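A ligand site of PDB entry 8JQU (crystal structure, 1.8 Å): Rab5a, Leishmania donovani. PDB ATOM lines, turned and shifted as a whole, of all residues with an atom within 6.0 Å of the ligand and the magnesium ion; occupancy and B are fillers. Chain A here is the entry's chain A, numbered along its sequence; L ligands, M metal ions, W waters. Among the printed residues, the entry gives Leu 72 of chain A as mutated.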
ATOM      1  N   GLY A  20      18.907  15.146  -8.862  1.00  0.00           N
ATOM      2  CA  GLY A  20      17.635  15.797  -8.645  1.00  0.00           C
ATOM      3  C   GLY A  20      16.482  14.839  -8.980  1.00  0.00           C
ATOM      4  O   GLY A  20      16.671  13.773  -9.541  1.00  0.00           O
ATOM      5  N   GLU A  21      15.273  15.310  -8.688  1.00  0.00           N
ATOM      6  CA  GLU A  21      14.106  14.425  -8.780  1.00  0.00           C
ATOM      7  C   GLU A  21      13.945  13.930 -10.219  1.00  0.00           C
ATOM      8  O   GLU A  21      14.232  14.619 -11.222  1.00  0.00           O
ATOM      9  CB  GLU A  21      12.913  15.311  -8.473  1.00  0.00           C
ATOM     10  CG  GLU A  21      11.644  14.447  -8.452  1.00  0.00           C
ATOM     11  CD  GLU A  21      10.434  15.167  -7.960  1.00  0.00           C
ATOM     12  OE1 GLU A  21       9.767  14.635  -7.086  1.00  0.00           O
ATOM     13  OE2 GLU A  21      10.131  16.224  -8.530  1.00  0.00           O
ATOM     14  N   SER A  22      13.429  12.705 -10.367  1.00  0.00           N
ATOM     15  CA  SER A  22      13.168  12.175 -11.709  1.00  0.00           C
ATOM     16  C   SER A  22      12.183  13.056 -12.454  1.00  0.00           C
ATOM     17  O   SER A  22      11.210  13.614 -11.860  1.00  0.00           O
ATOM     18  CB  SER A  22      12.604  10.688 -11.568  1.00  0.00           C
ATOM     19  OG  SER A  22      12.159  10.213 -12.810  1.00  0.00           O
ATOM     20  N   GLY A  23      12.424  13.218 -13.761  1.00  0.00           N
ATOM     21  CA  GLY A  23      11.536  14.041 -14.575  1.00  0.00           C
ATOM     22  C   GLY A  23      11.927  15.532 -14.610  1.00  0.00           C
ATOM     23  O   GLY A  23      11.347  16.279 -15.376  1.00  0.00           O
ATOM     24  N   ALA A  24      12.832  16.023 -13.738  1.00  0.00           N
ATOM     25  CA  ALA A  24      13.097  17.452 -13.763  1.00  0.00           C
ATOM     26  C   ALA A  24      13.854  17.875 -15.024  1.00  0.00           C
ATOM     27  O   ALA A  24      13.817  19.077 -15.413  1.00  0.00           O
ATOM     28  CB  ALA A  24      13.896  17.866 -12.540  1.00  0.00           C
ATOM     29  N   GLY A  25      14.625  16.934 -15.619  1.00  0.00           N
ATOM     30  CA  GLY A  25      15.310  17.247 -16.873  1.00  0.00           C
ATOM     31  C   GLY A  25      16.846  17.142 -16.780  1.00  0.00           C
ATOM     32  O   GLY A  25      17.535  17.733 -17.599  1.00  0.00           O
ATOM     33  N   LYS A  26      17.357  16.239 -15.946  1.00  0.00           N
ATOM     34  CA  LYS A  26      18.811  16.113 -15.784  1.00  0.00           C
ATOM     35  C   LYS A  26      19.425  15.658 -17.115  1.00  0.00           C
ATOM     36  O   LYS A  26      20.413  16.226 -17.621  1.00  0.00           O
ATOM     37  CB  LYS A  26      19.121  15.099 -14.651  1.00  0.00           C
ATOM     38  CG  LYS A  26      18.864  15.633 -13.221  1.00  0.00           C
ATOM     39  CD  LYS A  26      19.123  14.562 -12.226  1.00  0.00           C
ATOM     40  CE  LYS A  26      18.415  13.230 -12.476  1.00  0.00           C
ATOM     41  NZ  LYS A  26      16.951  13.427 -12.424  1.00  0.00           N
ATOM     42  N   SER A  27      18.821  14.606 -17.698  1.00  0.00           N
ATOM     43  CA  SER A  27      19.380  14.063 -18.922  1.00  0.00           C
ATOM     44  C   SER A  27      19.206  15.062 -20.071  1.00  0.00           C
ATOM     45  O   SER A  27      20.107  15.221 -20.910  1.00  0.00           O
ATOM     46  CB  SER A  27      18.687  12.747 -19.257  1.00  0.00           C
ATOM     47  OG  SER A  27      18.873  11.780 -18.210  1.00  0.00           O
ATOM     48  N   SER A  28      18.065  15.764 -20.070  1.00  0.00           N
ATOM     49  CA  SER A  28      17.841  16.725 -21.151  1.00  0.00           C
ATOM     50  C   SER A  28      18.861  17.852 -21.106  1.00  0.00           C
ATOM     51  O   SER A  28      19.365  18.292 -22.152  1.00  0.00           O
ATOM     52  CB  SER A  28      16.432  17.262 -21.092  1.00  0.00           C
ATOM     53  OG  SER A  28      15.477  16.190 -21.290  1.00  0.00           O
ATOM     54  N   ILE A  29      19.127  18.354 -19.905  1.00  0.00           N
ATOM     55  CA  ILE A  29      20.140  19.418 -19.827  1.00  0.00           C
ATOM     56  C   ILE A  29      21.498  18.887 -20.301  1.00  0.00           C
ATOM     57  O   ILE A  29      22.236  19.564 -21.028  1.00  0.00           O
ATOM     58  CB  ILE A  29      20.210  19.926 -18.358  1.00  0.00           C
ATOM     59  CG1 ILE A  29      18.923  20.721 -18.048  1.00  0.00           C
ATOM     60  CG2 ILE A  29      21.503  20.732 -18.063  1.00  0.00           C
ATOM     61  CD1 ILE A  29      18.736  20.974 -16.499  1.00  0.00           C
ATOM     62  N   PHE A  38      17.935  17.083 -27.786  1.00  0.00           N
ATOM     63  CA  PHE A  38      16.803  17.115 -26.866  1.00  0.00           C
ATOM     64  C   PHE A  38      15.731  16.171 -27.384  1.00  0.00           C
ATOM     65  O   PHE A  38      15.460  16.117 -28.604  1.00  0.00           O
ATOM     66  CB  PHE A  38      16.226  18.545 -26.832  1.00  0.00           C
ATOM     67  CG  PHE A  38      15.001  18.648 -25.937  1.00  0.00           C
ATOM     68  CD1 PHE A  38      15.152  18.683 -24.552  1.00  0.00           C
ATOM     69  CD2 PHE A  38      13.706  18.605 -26.478  1.00  0.00           C
ATOM     70  CE1 PHE A  38      14.019  18.732 -23.734  1.00  0.00           C
ATOM     71  CE2 PHE A  38      12.566  18.620 -25.636  1.00  0.00           C
ATOM     72  CZ  PHE A  38      12.719  18.694 -24.269  1.00  0.00           C
ATOM     73  N   LEU A  39      15.112  15.395 -26.497  1.00  0.00           N
ATOM     74  CA  LEU A  39      14.020  14.506 -26.915  1.00  0.00           C
ATOM     75  C   LEU A  39      12.782  14.810 -26.062  1.00  0.00           C
ATOM     76  O   LEU A  39      12.850  14.776 -24.804  1.00  0.00           O
ATOM     77  CB  LEU A  39      14.459  13.057 -26.701  1.00  0.00           C
ATOM     78  CG  LEU A  39      15.563  12.540 -27.640  1.00  0.00           C
ATOM     79  CD1 LEU A  39      16.057  11.207 -27.149  1.00  0.00           C
ATOM     80  CD2 LEU A  39      14.996  12.382 -29.055  1.00  0.00           C
ATOM     81  N   ALA A  40      11.626  15.062 -26.725  1.00  0.00           N
ATOM     82  CA  ALA A  40      10.358  15.250 -26.001  1.00  0.00           C
ATOM     83  C   ALA A  40      10.003  13.997 -25.208  1.00  0.00           C
ATOM     84  O   ALA A  40       9.293  14.079 -24.200  1.00  0.00           O
ATOM     85  CB  ALA A  40       9.215  15.621 -26.945  1.00  0.00           C
ATOM     86  N   ASN A  41      10.527  12.829 -25.652  1.00  0.00           N
ATOM     87  CA  ASN A  41      10.228  11.571 -24.966  1.00  0.00           C
ATOM     88  C   ASN A  41      11.436  10.909 -24.338  1.00  0.00           C
ATOM     89  O   ASN A  41      11.518   9.691 -24.278  1.00  0.00           O
ATOM     90  CB  ASN A  41       9.632  10.551 -25.958  1.00  0.00           C
ATOM     91  CG  ASN A  41       8.237  10.968 -26.338  1.00  0.00           C
ATOM     92  OD1 ASN A  41       7.421  11.311 -25.489  1.00  0.00           O
ATOM     93  ND2 ASN A  41       7.938  10.942 -27.629  1.00  0.00           N
ATOM     94  N   GLN A  42      12.416  11.710 -23.906  1.00  0.00           N
ATOM     95  CA  GLN A  42      13.630  11.205 -23.277  1.00  0.00           C
ATOM     96  C   GLN A  42      13.227  10.083 -22.294  1.00  0.00           C
ATOM     97  O   GLN A  42      12.388  10.338 -21.440  1.00  0.00           O
ATOM     98  CB  GLN A  42      14.350  12.363 -22.552  1.00  0.00           C
ATOM     99  CG  GLN A  42      15.775  12.009 -22.044  1.00  0.00           C
ATOM    100  CD  GLN A  42      16.751  11.909 -23.202  1.00  0.00           C
ATOM    101  OE1 GLN A  42      16.839  12.773 -24.075  1.00  0.00           O
ATOM    102  NE2 GLN A  42      17.470  10.808 -23.231  1.00  0.00           N
ATOM    103  N   GLU A  43      13.856   8.904 -22.415  1.00  0.00           N
ATOM    104  CA  GLU A  43      13.561   7.783 -21.526  1.00  0.00           C
ATOM    105  C   GLU A  43      14.137   7.974 -20.112  1.00  0.00           C
ATOM    106  O   GLU A  43      15.256   8.469 -19.956  1.00  0.00           O
ATOM    107  CB  GLU A  43      14.105   6.481 -22.134  1.00  0.00           C
ATOM    108  CG  GLU A  43      13.265   5.967 -23.275  1.00  0.00           C
ATOM    109  CD  GLU A  43      13.882   4.765 -23.982  1.00  0.00           C
ATOM    110  N   THR A  44      13.391   7.588 -19.061  1.00  0.00           N
ATOM    111  CA  THR A  44      13.918   7.689 -17.703  1.00  0.00           C
ATOM    112  C   THR A  44      15.262   6.937 -17.601  1.00  0.00           C
ATOM    113  O   THR A  44      15.430   5.837 -18.170  1.00  0.00           O
ATOM    114  CB  THR A  44      12.837   7.256 -16.685  1.00  0.00           C
ATOM    115  OG1 THR A  44      13.332   7.414 -15.344  1.00  0.00           O
ATOM    116  CG2 THR A  44      12.348   5.848 -16.928  1.00  0.00           C
ATOM    117  N   THR A  45      16.221   7.503 -16.843  1.00  0.00           N
ATOM    118  CA  THR A  45      17.589   6.961 -16.821  1.00  0.00           C
ATOM    119  C   THR A  45      17.608   5.783 -15.841  1.00  0.00           C
ATOM    120  O   THR A  45      17.160   5.934 -14.726  1.00  0.00           O
ATOM    121  CB  THR A  45      18.556   8.054 -16.358  1.00  0.00           C
ATOM    122  OG1 THR A  45      18.461   9.098 -17.328  1.00  0.00           O
ATOM    123  CG2 THR A  45      20.024   7.661 -16.264  1.00  0.00           C
ATOM    124  N   ILE A  46      18.172   4.659 -16.283  1.00  0.00           N
ATOM    125  CA  ILE A  46      18.258   3.480 -15.438  1.00  0.00           C
ATOM    126  C   ILE A  46      19.631   3.503 -14.763  1.00  0.00           C
ATOM    127  O   ILE A  46      19.782   3.650 -13.531  1.00  0.00           O
ATOM    128  CB  ILE A  46      17.978   2.200 -16.294  1.00  0.00           C
ATOM    129  CG1 ILE A  46      16.525   2.135 -16.776  1.00  0.00           C
ATOM    130  CG2 ILE A  46      18.376   0.919 -15.578  1.00  0.00           C
ATOM    131  CD1 ILE A  46      15.532   2.656 -15.744  1.00  0.00           C
ATOM    132  N   ASP A  68      25.349  11.618 -15.449  1.00  0.00           N
ATOM    133  CA  ASP A  68      23.915  11.937 -15.425  1.00  0.00           C
ATOM    134  C   ASP A  68      23.198  10.848 -14.644  1.00  0.00           C
ATOM    135  O   ASP A  68      23.069   9.689 -15.111  1.00  0.00           O
ATOM    136  CB  ASP A  68      23.470  12.021 -16.880  1.00  0.00           C
ATOM    137  CG  ASP A  68      21.978  12.128 -17.031  1.00  0.00           C
ATOM    138  OD1 ASP A  68      21.355  12.656 -16.080  1.00  0.00           O
ATOM    139  OD2 ASP A  68      21.431  11.590 -18.067  1.00  0.00           O
ATOM    140  N   THR A  69      22.915  11.115 -13.359  1.00  0.00           N
ATOM    141  CA  THR A  69      22.355  10.033 -12.559  1.00  0.00           C
ATOM    142  C   THR A  69      20.849   9.793 -12.803  1.00  0.00           C
ATOM    143  O   THR A  69      20.073  10.663 -13.169  1.00  0.00           O
ATOM    144  CB  THR A  69      22.690  10.222 -11.055  1.00  0.00           C
ATOM    145  OG1 THR A  69      21.844  11.317 -10.641  1.00  0.00           O
ATOM    146  CG2 THR A  69      24.122  10.620 -10.742  1.00  0.00           C
ATOM    147  N   ALA A  70      20.403   8.557 -12.511  1.00  0.00           N
ATOM    148  CA  ALA A  70      18.986   8.227 -12.427  1.00  0.00           C
ATOM    149  C   ALA A  70      18.365   8.879 -11.178  1.00  0.00           C
ATOM    150  O   ALA A  70      18.853   8.673 -10.042  1.00  0.00           O
ATOM    151  CB  ALA A  70      18.829   6.725 -12.310  1.00  0.00           C
ATOM    152  N   GLY A  71      17.256   9.623 -11.334  1.00  0.00           N
ATOM    153  CA  GLY A  71      16.714  10.397 -10.214  1.00  0.00           C
ATOM    154  C   GLY A  71      15.672   9.651  -9.349  1.00  0.00           C
ATOM    155  O   GLY A  71      15.247  10.160  -8.312  1.00  0.00           O
ATOM    156  N   LEU A  72      15.177   8.525  -9.854  1.00  0.00           N
ATOM    157  CA  LEU A  72      14.140   7.793  -9.133  1.00  0.00           C
ATOM    158  C   LEU A  72      14.690   7.403  -7.751  1.00  0.00           C
ATOM    159  O   LEU A  72      15.874   7.115  -7.604  1.00  0.00           O
ATOM    160  CB  LEU A  72      13.693   6.566  -9.937  1.00  0.00           C
ATOM    161  CG  LEU A  72      12.644   6.871 -11.013  1.00  0.00           C
ATOM    162  CD1 LEU A  72      12.391   5.648 -11.892  1.00  0.00           C
ATOM    163  CD2 LEU A  72      11.328   7.401 -10.426  1.00  0.00           C
ATOM    164  N   ASN A 126      14.657  24.020 -14.094  1.00  0.00           N
ATOM    165  CA  ASN A 126      14.551  23.745 -15.538  1.00  0.00           C
ATOM    166  C   ASN A 126      13.084  23.825 -15.963  1.00  0.00           C
ATOM    167  O   ASN A 126      12.185  23.974 -15.143  1.00  0.00           O
ATOM    168  CB  ASN A 126      15.128  22.322 -15.816  1.00  0.00           C
ATOM    169  CG  ASN A 126      15.146  21.950 -17.299  1.00  0.00           C
ATOM    170  OD1 ASN A 126      15.524  22.793 -18.125  1.00  0.00           O
ATOM    171  ND2 ASN A 126      14.773  20.710 -17.641  1.00  0.00           N
ATOM    172  N   LYS A 127      12.891  23.812 -17.291  1.00  0.00           N
ATOM    173  CA  LYS A 127      11.585  23.931 -17.955  1.00  0.00           C
ATOM    174  C   LYS A 127      10.986  25.325 -17.878  1.00  0.00           C
ATOM    175  O   LYS A 127       9.769  25.435 -17.813  1.00  0.00           O
ATOM    176  CB  LYS A 127      10.546  22.923 -17.397  1.00  0.00           C
ATOM    177  CG  LYS A 127      11.070  21.482 -17.322  1.00  0.00           C
ATOM    178  CD  LYS A 127       9.964  20.402 -17.210  1.00  0.00           C
ATOM    179  CE  LYS A 127      10.623  19.014 -17.094  1.00  0.00           C
ATOM    180  NZ  LYS A 127       9.601  17.929 -17.128  1.00  0.00           N
ATOM    181  N   LYS A 128      11.838  26.352 -17.969  1.00  0.00           N
ATOM    182  CA  LYS A 128      11.385  27.724 -17.906  1.00  0.00           C
ATOM    183  C   LYS A 128      10.448  27.998 -19.093  1.00  0.00           C
ATOM    184  O   LYS A 128       9.672  28.935 -19.042  1.00  0.00           O
ATOM    185  CB  LYS A 128      12.652  28.591 -17.949  1.00  0.00           C
ATOM    186  CG  LYS A 128      12.435  30.100 -17.866  1.00  0.00           C
ATOM    187  CD  LYS A 128      13.785  30.823 -17.828  1.00  0.00           C
ATOM    188  CE  LYS A 128      14.816  30.415 -18.872  1.00  0.00           C
ATOM    189  N   ASP A 129      10.523  27.199 -20.166  1.00  0.00           N
ATOM    190  CA  ASP A 129       9.725  27.443 -21.368  1.00  0.00           C
ATOM    191  C   ASP A 129       8.222  27.197 -21.110  1.00  0.00           C
ATOM    192  O   ASP A 129       7.345  27.568 -21.947  1.00  0.00           O
ATOM    193  CB  ASP A 129      10.218  26.540 -22.490  1.00  0.00           C
ATOM    194  CG  ASP A 129      10.170  25.066 -22.131  1.00  0.00           C
ATOM    195  OD1 ASP A 129      11.090  24.619 -21.368  1.00  0.00           O
ATOM    196  OD2 ASP A 129       9.183  24.378 -22.503  1.00  0.00           O
ATOM    197  N   LEU A 130       7.911  26.488 -20.029  1.00  0.00           N
ATOM    198  CA  LEU A 130       6.518  26.142 -19.719  1.00  0.00           C
ATOM    199  C   LEU A 130       5.897  27.278 -18.906  1.00  0.00           C
ATOM    200  O   LEU A 130       5.346  27.026 -17.841  1.00  0.00           O
ATOM    201  CB  LEU A 130       6.397  24.801 -18.945  1.00  0.00           C
ATOM    202  CG  LEU A 130       6.878  23.575 -19.754  1.00  0.00           C
ATOM    203  CD1 LEU A 130       6.701  22.309 -18.901  1.00  0.00           C
ATOM    204  CD2 LEU A 130       5.975  23.392 -21.005  1.00  0.00           C
ATOM    205  N   ALA A 156      16.558  27.631 -16.441  1.00  0.00           N
ATOM    206  CA  ALA A 156      16.993  27.283 -17.785  1.00  0.00           C
ATOM    207  C   ALA A 156      15.880  26.477 -18.472  1.00  0.00           C
ATOM    208  O   ALA A 156      14.830  26.163 -17.868  1.00  0.00           O
ATOM    209  CB  ALA A 156      18.234  26.382 -17.691  1.00  0.00           C
ATOM    210  N   SER A 157      16.112  26.190 -19.790  1.00  0.00           N
ATOM    211  CA  SER A 157      15.230  25.340 -20.571  1.00  0.00           C
ATOM    212  C   SER A 157      16.121  24.489 -21.480  1.00  0.00           C
ATOM    213  O   SER A 157      16.728  24.997 -22.446  1.00  0.00           O
ATOM    214  CB  SER A 157      14.264  26.182 -21.482  1.00  0.00           C
ATOM    215  OG  SER A 157      13.511  25.243 -22.252  1.00  0.00           O
ATOM    216  N   ALA A 158      16.213  23.186 -21.146  1.00  0.00           N
ATOM    217  CA  ALA A 158      16.822  22.239 -22.092  1.00  0.00           C
ATOM    218  C   ALA A 158      16.106  22.212 -23.424  1.00  0.00           C
ATOM    219  O   ALA A 158      16.747  22.115 -24.490  1.00  0.00           O
ATOM    220  CB  ALA A 158      16.808  20.823 -21.511  1.00  0.00           C
ATOM    221  N   LYS A 159      14.794  22.407 -23.365  1.00  0.00           N
ATOM    222  CA  LYS A 159      14.047  22.271 -24.613  1.00  0.00           C
ATOM    223  C   LYS A 159      14.412  23.438 -25.540  1.00  0.00           C
ATOM    224  O   LYS A 159      14.618  23.198 -26.759  1.00  0.00           O
ATOM    225  CB  LYS A 159      12.564  22.234 -24.285  1.00  0.00           C
ATOM    226  CG  LYS A 159      11.674  22.266 -25.545  1.00  0.00           C
ATOM    227  CD  LYS A 159      10.174  22.109 -25.194  1.00  0.00           C
ATOM    228  CE  LYS A 159       9.413  22.284 -26.500  1.00  0.00           C
ATOM    229  NZ  LYS A 159       8.014  21.864 -26.248  1.00  0.00           N
ATOM    230  N   ASP A 160      14.415  24.668 -24.996  1.00  0.00           N
ATOM    231  CA  ASP A 160      14.679  25.855 -25.824  1.00  0.00           C
ATOM    232  C   ASP A 160      16.174  26.156 -25.901  1.00  0.00           C
ATOM    233  O   ASP A 160      16.589  27.082 -26.593  1.00  0.00           O
ATOM    234  CB  ASP A 160      14.132  27.118 -25.184  1.00  0.00           C
ATOM    235  CG  ASP A 160      12.613  27.273 -25.235  1.00  0.00           C
ATOM    236  OD1 ASP A 160      11.975  26.497 -25.897  1.00  0.00           O
ATOM    237  OD2 ASP A 160      12.106  28.174 -24.465  1.00  0.00           O
HETATM  238  P1  LIG L   1      15.285  10.639 -14.672  1.00  0.00           P
HETATM  239  O1  LIG L   1      14.154   9.658 -14.436  1.00  0.00           O
HETATM  240  O2  LIG L   1      16.327  10.138 -15.620  1.00  0.00           O
HETATM  241  O3  LIG L   1      15.904  11.078 -13.403  1.00  0.00           O
HETATM  242  N1  LIG L   1      14.544  11.947 -15.429  1.00  0.00           N
HETATM  243  P2  LIG L   1      15.437  13.284 -15.893  1.00  0.00           P
HETATM  244  O4  LIG L   1      15.648  14.270 -14.827  1.00  0.00           O
HETATM  245  O5  LIG L   1      16.627  12.804 -16.637  1.00  0.00           O
HETATM  246  O6  LIG L   1      14.435  13.963 -16.967  1.00  0.00           O
HETATM  247  P3  LIG L   1      14.480  13.920 -18.582  1.00  0.00           P
HETATM  248  O7  LIG L   1      15.621  14.688 -19.142  1.00  0.00           O
HETATM  249  O8  LIG L   1      14.303  12.464 -18.951  1.00  0.00           O
HETATM  250  O9  LIG L   1      13.146  14.725 -18.924  1.00  0.00           O
HETATM  251  C1  LIG L   1      11.849  14.275 -18.456  1.00  0.00           C
HETATM  252  C2  LIG L   1      10.832  14.842 -19.429  1.00  0.00           C
HETATM  253  O10 LIG L   1      10.858  16.295 -19.366  1.00  0.00           O
HETATM  254  C3  LIG L   1      11.048  14.467 -20.907  1.00  0.00           C
HETATM  255  O11 LIG L   1       9.765  14.307 -21.501  1.00  0.00           O
HETATM  256  C4  LIG L   1      11.709  15.721 -21.501  1.00  0.00           C
HETATM  257  O12 LIG L   1      11.408  15.967 -22.852  1.00  0.00           O
HETATM  258  C5  LIG L   1      11.085  16.831 -20.651  1.00  0.00           C
HETATM  259  N2  LIG L   1      11.920  18.027 -20.537  1.00  0.00           N
HETATM  260  C6  LIG L   1      13.211  18.104 -20.063  1.00  0.00           C
HETATM  261  N3  LIG L   1      13.692  19.327 -20.120  1.00  0.00           N
HETATM  262  C7  LIG L   1      12.626  20.109 -20.539  1.00  0.00           C
HETATM  263  C8  LIG L   1      12.540  21.523 -20.746  1.00  0.00           C
HETATM  264  O13 LIG L   1      13.416  22.371 -20.581  1.00  0.00           O
HETATM  265  N4  LIG L   1      11.247  21.916 -21.117  1.00  0.00           N
HETATM  266  C9  LIG L   1      10.197  21.037 -21.331  1.00  0.00           C
HETATM  267  N5  LIG L   1       9.026  21.564 -21.748  1.00  0.00           N
HETATM  268  N6  LIG L   1      10.292  19.711 -21.195  1.00  0.00           N
HETATM  269  C10 LIG L   1      11.524  19.317 -20.767  1.00  0.00           C
HETATM  270 MG    MG M   1      17.532  10.994 -16.924  1.00  0.00          MG
HETATM  271  O   HOH W   1       9.078  17.774 -23.636  1.00  0.00           O
HETATM  272  O   HOH W   2      15.437   7.702 -12.855  1.00  0.00           O
HETATM  273  O   HOH W   3       8.171  18.218 -19.657  1.00  0.00           O
HETATM  274  O   HOH W   4      18.937  11.448 -15.516  1.00  0.00           O
HETATM  275  O   HOH W   5       7.290  15.508 -20.683  1.00  0.00           O
HETATM  276  O   HOH W   6       6.546  20.093 -22.150  1.00  0.00           O
HETATM  277  O   HOH W   7      16.275  10.682 -18.560  1.00  0.00           O
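An oxygen (O5) of the ligand lies close to the backbone NH of Ser 27 (3.0 Å). An oxygen (O2) of the ligand lies close to the backbone NH (N) of Thr 45 (2.9 Å). OG1 of Thr 44 sits at hydrogen-bond distance from O1 of the ligand (2.6 Å). The backbone NH of Ser 28 lies within hydrogen-bond range of an oxygen (O7) of the ligand, 2.8 Å away. OG of Ser 28 is in hydrogen-bond range of O7 of the ligand, 2.6 Å away. OG of Ser 22 is in hydrogen-bond range of O1 of the ligand (2.6 Å). An oxygen (O12) of the ligand is in hydrogen-bond range of the backbone carbonyl oxygen (O) of Leu 39, 2.7 Å away. N4 of the ligand sits at hydrogen-bond distance from OD1 of Asp 129, at 2.7 Å. O of Ala 40 is in hydrogen-bond range of O11 of the ligand (2.7 Å). The backbone NH (N) of Lys 26 lies within hydrogen-bond range of an oxygen (O4) of the ligand (2.8 Å). An oxygen (O3) of the ligand is in salt-bridge range of the side-chain amino group of Lys 26, 2.8 Å away. O3 of the ligand is in hydrogen-bond range of N of Gly 71, 2.9 Å away. N of Gly 25 is in hydrogen-bond range of O4 of the ligand (3.0 Å). The backbone NH (N) of Ala 158 lies within hydrogen-bond range of an oxygen (O13) of the ligand. The side-chain amide nitrogen (ND2) of Asn 126 lies within hydrogen-bond range of a nitrogen (N3) of the ligand, 3.0 Å away. The side-chain amino group (NZ) of Lys 127 lies within hydrogen-bond range of an oxygen (O10) of the ligand, at 3.0 Å. An oxygen (O13) of the ligand sits at hydrogen-bond distance from the backbone NH (N) of Lys 159 (3.1 Å). The side-chain hydroxyl (OG) of Ser 157 is in hydrogen-bond range of an oxygen (O13) of the ligand. An oxygen (O4) of the ligand lies within hydrogen-bond range of the backbone NH (N) of Ala 24 (3.5 Å).
The side-chain carboxylate of Asp 68 lies close to the side-chain hydroxyl of Ser 27. OG of Ser 157 is in hydrogen-bond range of OD1 of Asp 129. NZ of Lys 26 lies within hydrogen-bond range of O of Glu 21. The side-chain amino group (NZ) of Lys 26 sits at hydrogen-bond distance from the backbone carbonyl oxygen (O) of Gly 20. OD1 of Asn 126 sits at hydrogen-bond distance from N of Ala 158 (3.1 Å). The backbone carbonyl oxygen (O) of Gly 23 lies within hydrogen-bond range of the side-chain amino group (NZ) of Lys 127, at 3.0 Å. ND2 of Asn 126 is in hydrogen-bond range of O of Ala 24 (2.9 Å). OD1 of Asn 126 sits close to O of Ala 156 (3.5 Å).
The backbone NH (N) of Gly 23 lies close to a nitrogen (N1) of the ligand, 3.0 Å away. Glu 21 touches the ligand (O to O4, 3.9 Å). Phe 38 touches the ligand (CZ to O12, 3.3 Å). Gln 42 touches the ligand. C of Ala 70 touches O3 of the ligand (3.98 Å). Leu 130 touches the ligand (CG to N5, 3.6 Å). 23 residues have an atom within 4 Å of the ligand: Glu 21, Ser 22, Gly 23, Ala 24, Gly 25, Lys 26, Ser 27, Ser 28, Phe 38, Leu 39, Ala 40, Gln 42, Thr 44, Thr 45, Ala 70, Gly 71, Asn 126, Lys 127, Asp 129, Leu 130, Ser 157, Ala 158 and Lys 159. Along chain A the residues within 4 Å of the ligand span positions 21 to 159.
Of the 34 residues printed, 2 come within 4 Å of the magnesium ion. The nearest printed residue that does not touch the magnesium ion is Asp 68 (4.1 Å).
The magnesium ion is bound by an oxygen (O2) of the ligand (2.0 Å), the side-chain hydroxyl (OG) of Ser 27 (2.0 Å), water W4 (2.0 Å), an oxygen (O5) of the ligand (2.0 Å), water W7 (2.1 Å) and the side-chain hydroxyl (OG1) of Thr 45 (2.1 Å). The magnesium ion has six donor atoms within binding distance.
Water W7 bridges O8 of the ligand (2.7 Å) and O of Glu 43 (2.8 Å). Water W4 lies within hydrogen-bond range of the backbone carbonyl oxygen of Thr 69 and the side-chain carboxylate of Asp 68. Water W2 lies within hydrogen-bond range of an oxygen (O1) of the ligand, the backbone NH (N) of Gly 71, the backbone carbonyl oxygen (O) of Thr 45, the backbone NH (N) of Leu 72 and the side-chain hydroxyl (OG1) of Thr 44. Water W3 bridges the side-chain amino group (NZ) of Lys 127 (2.9 Å) and a nitrogen (N6) of the ligand (3.0 Å).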
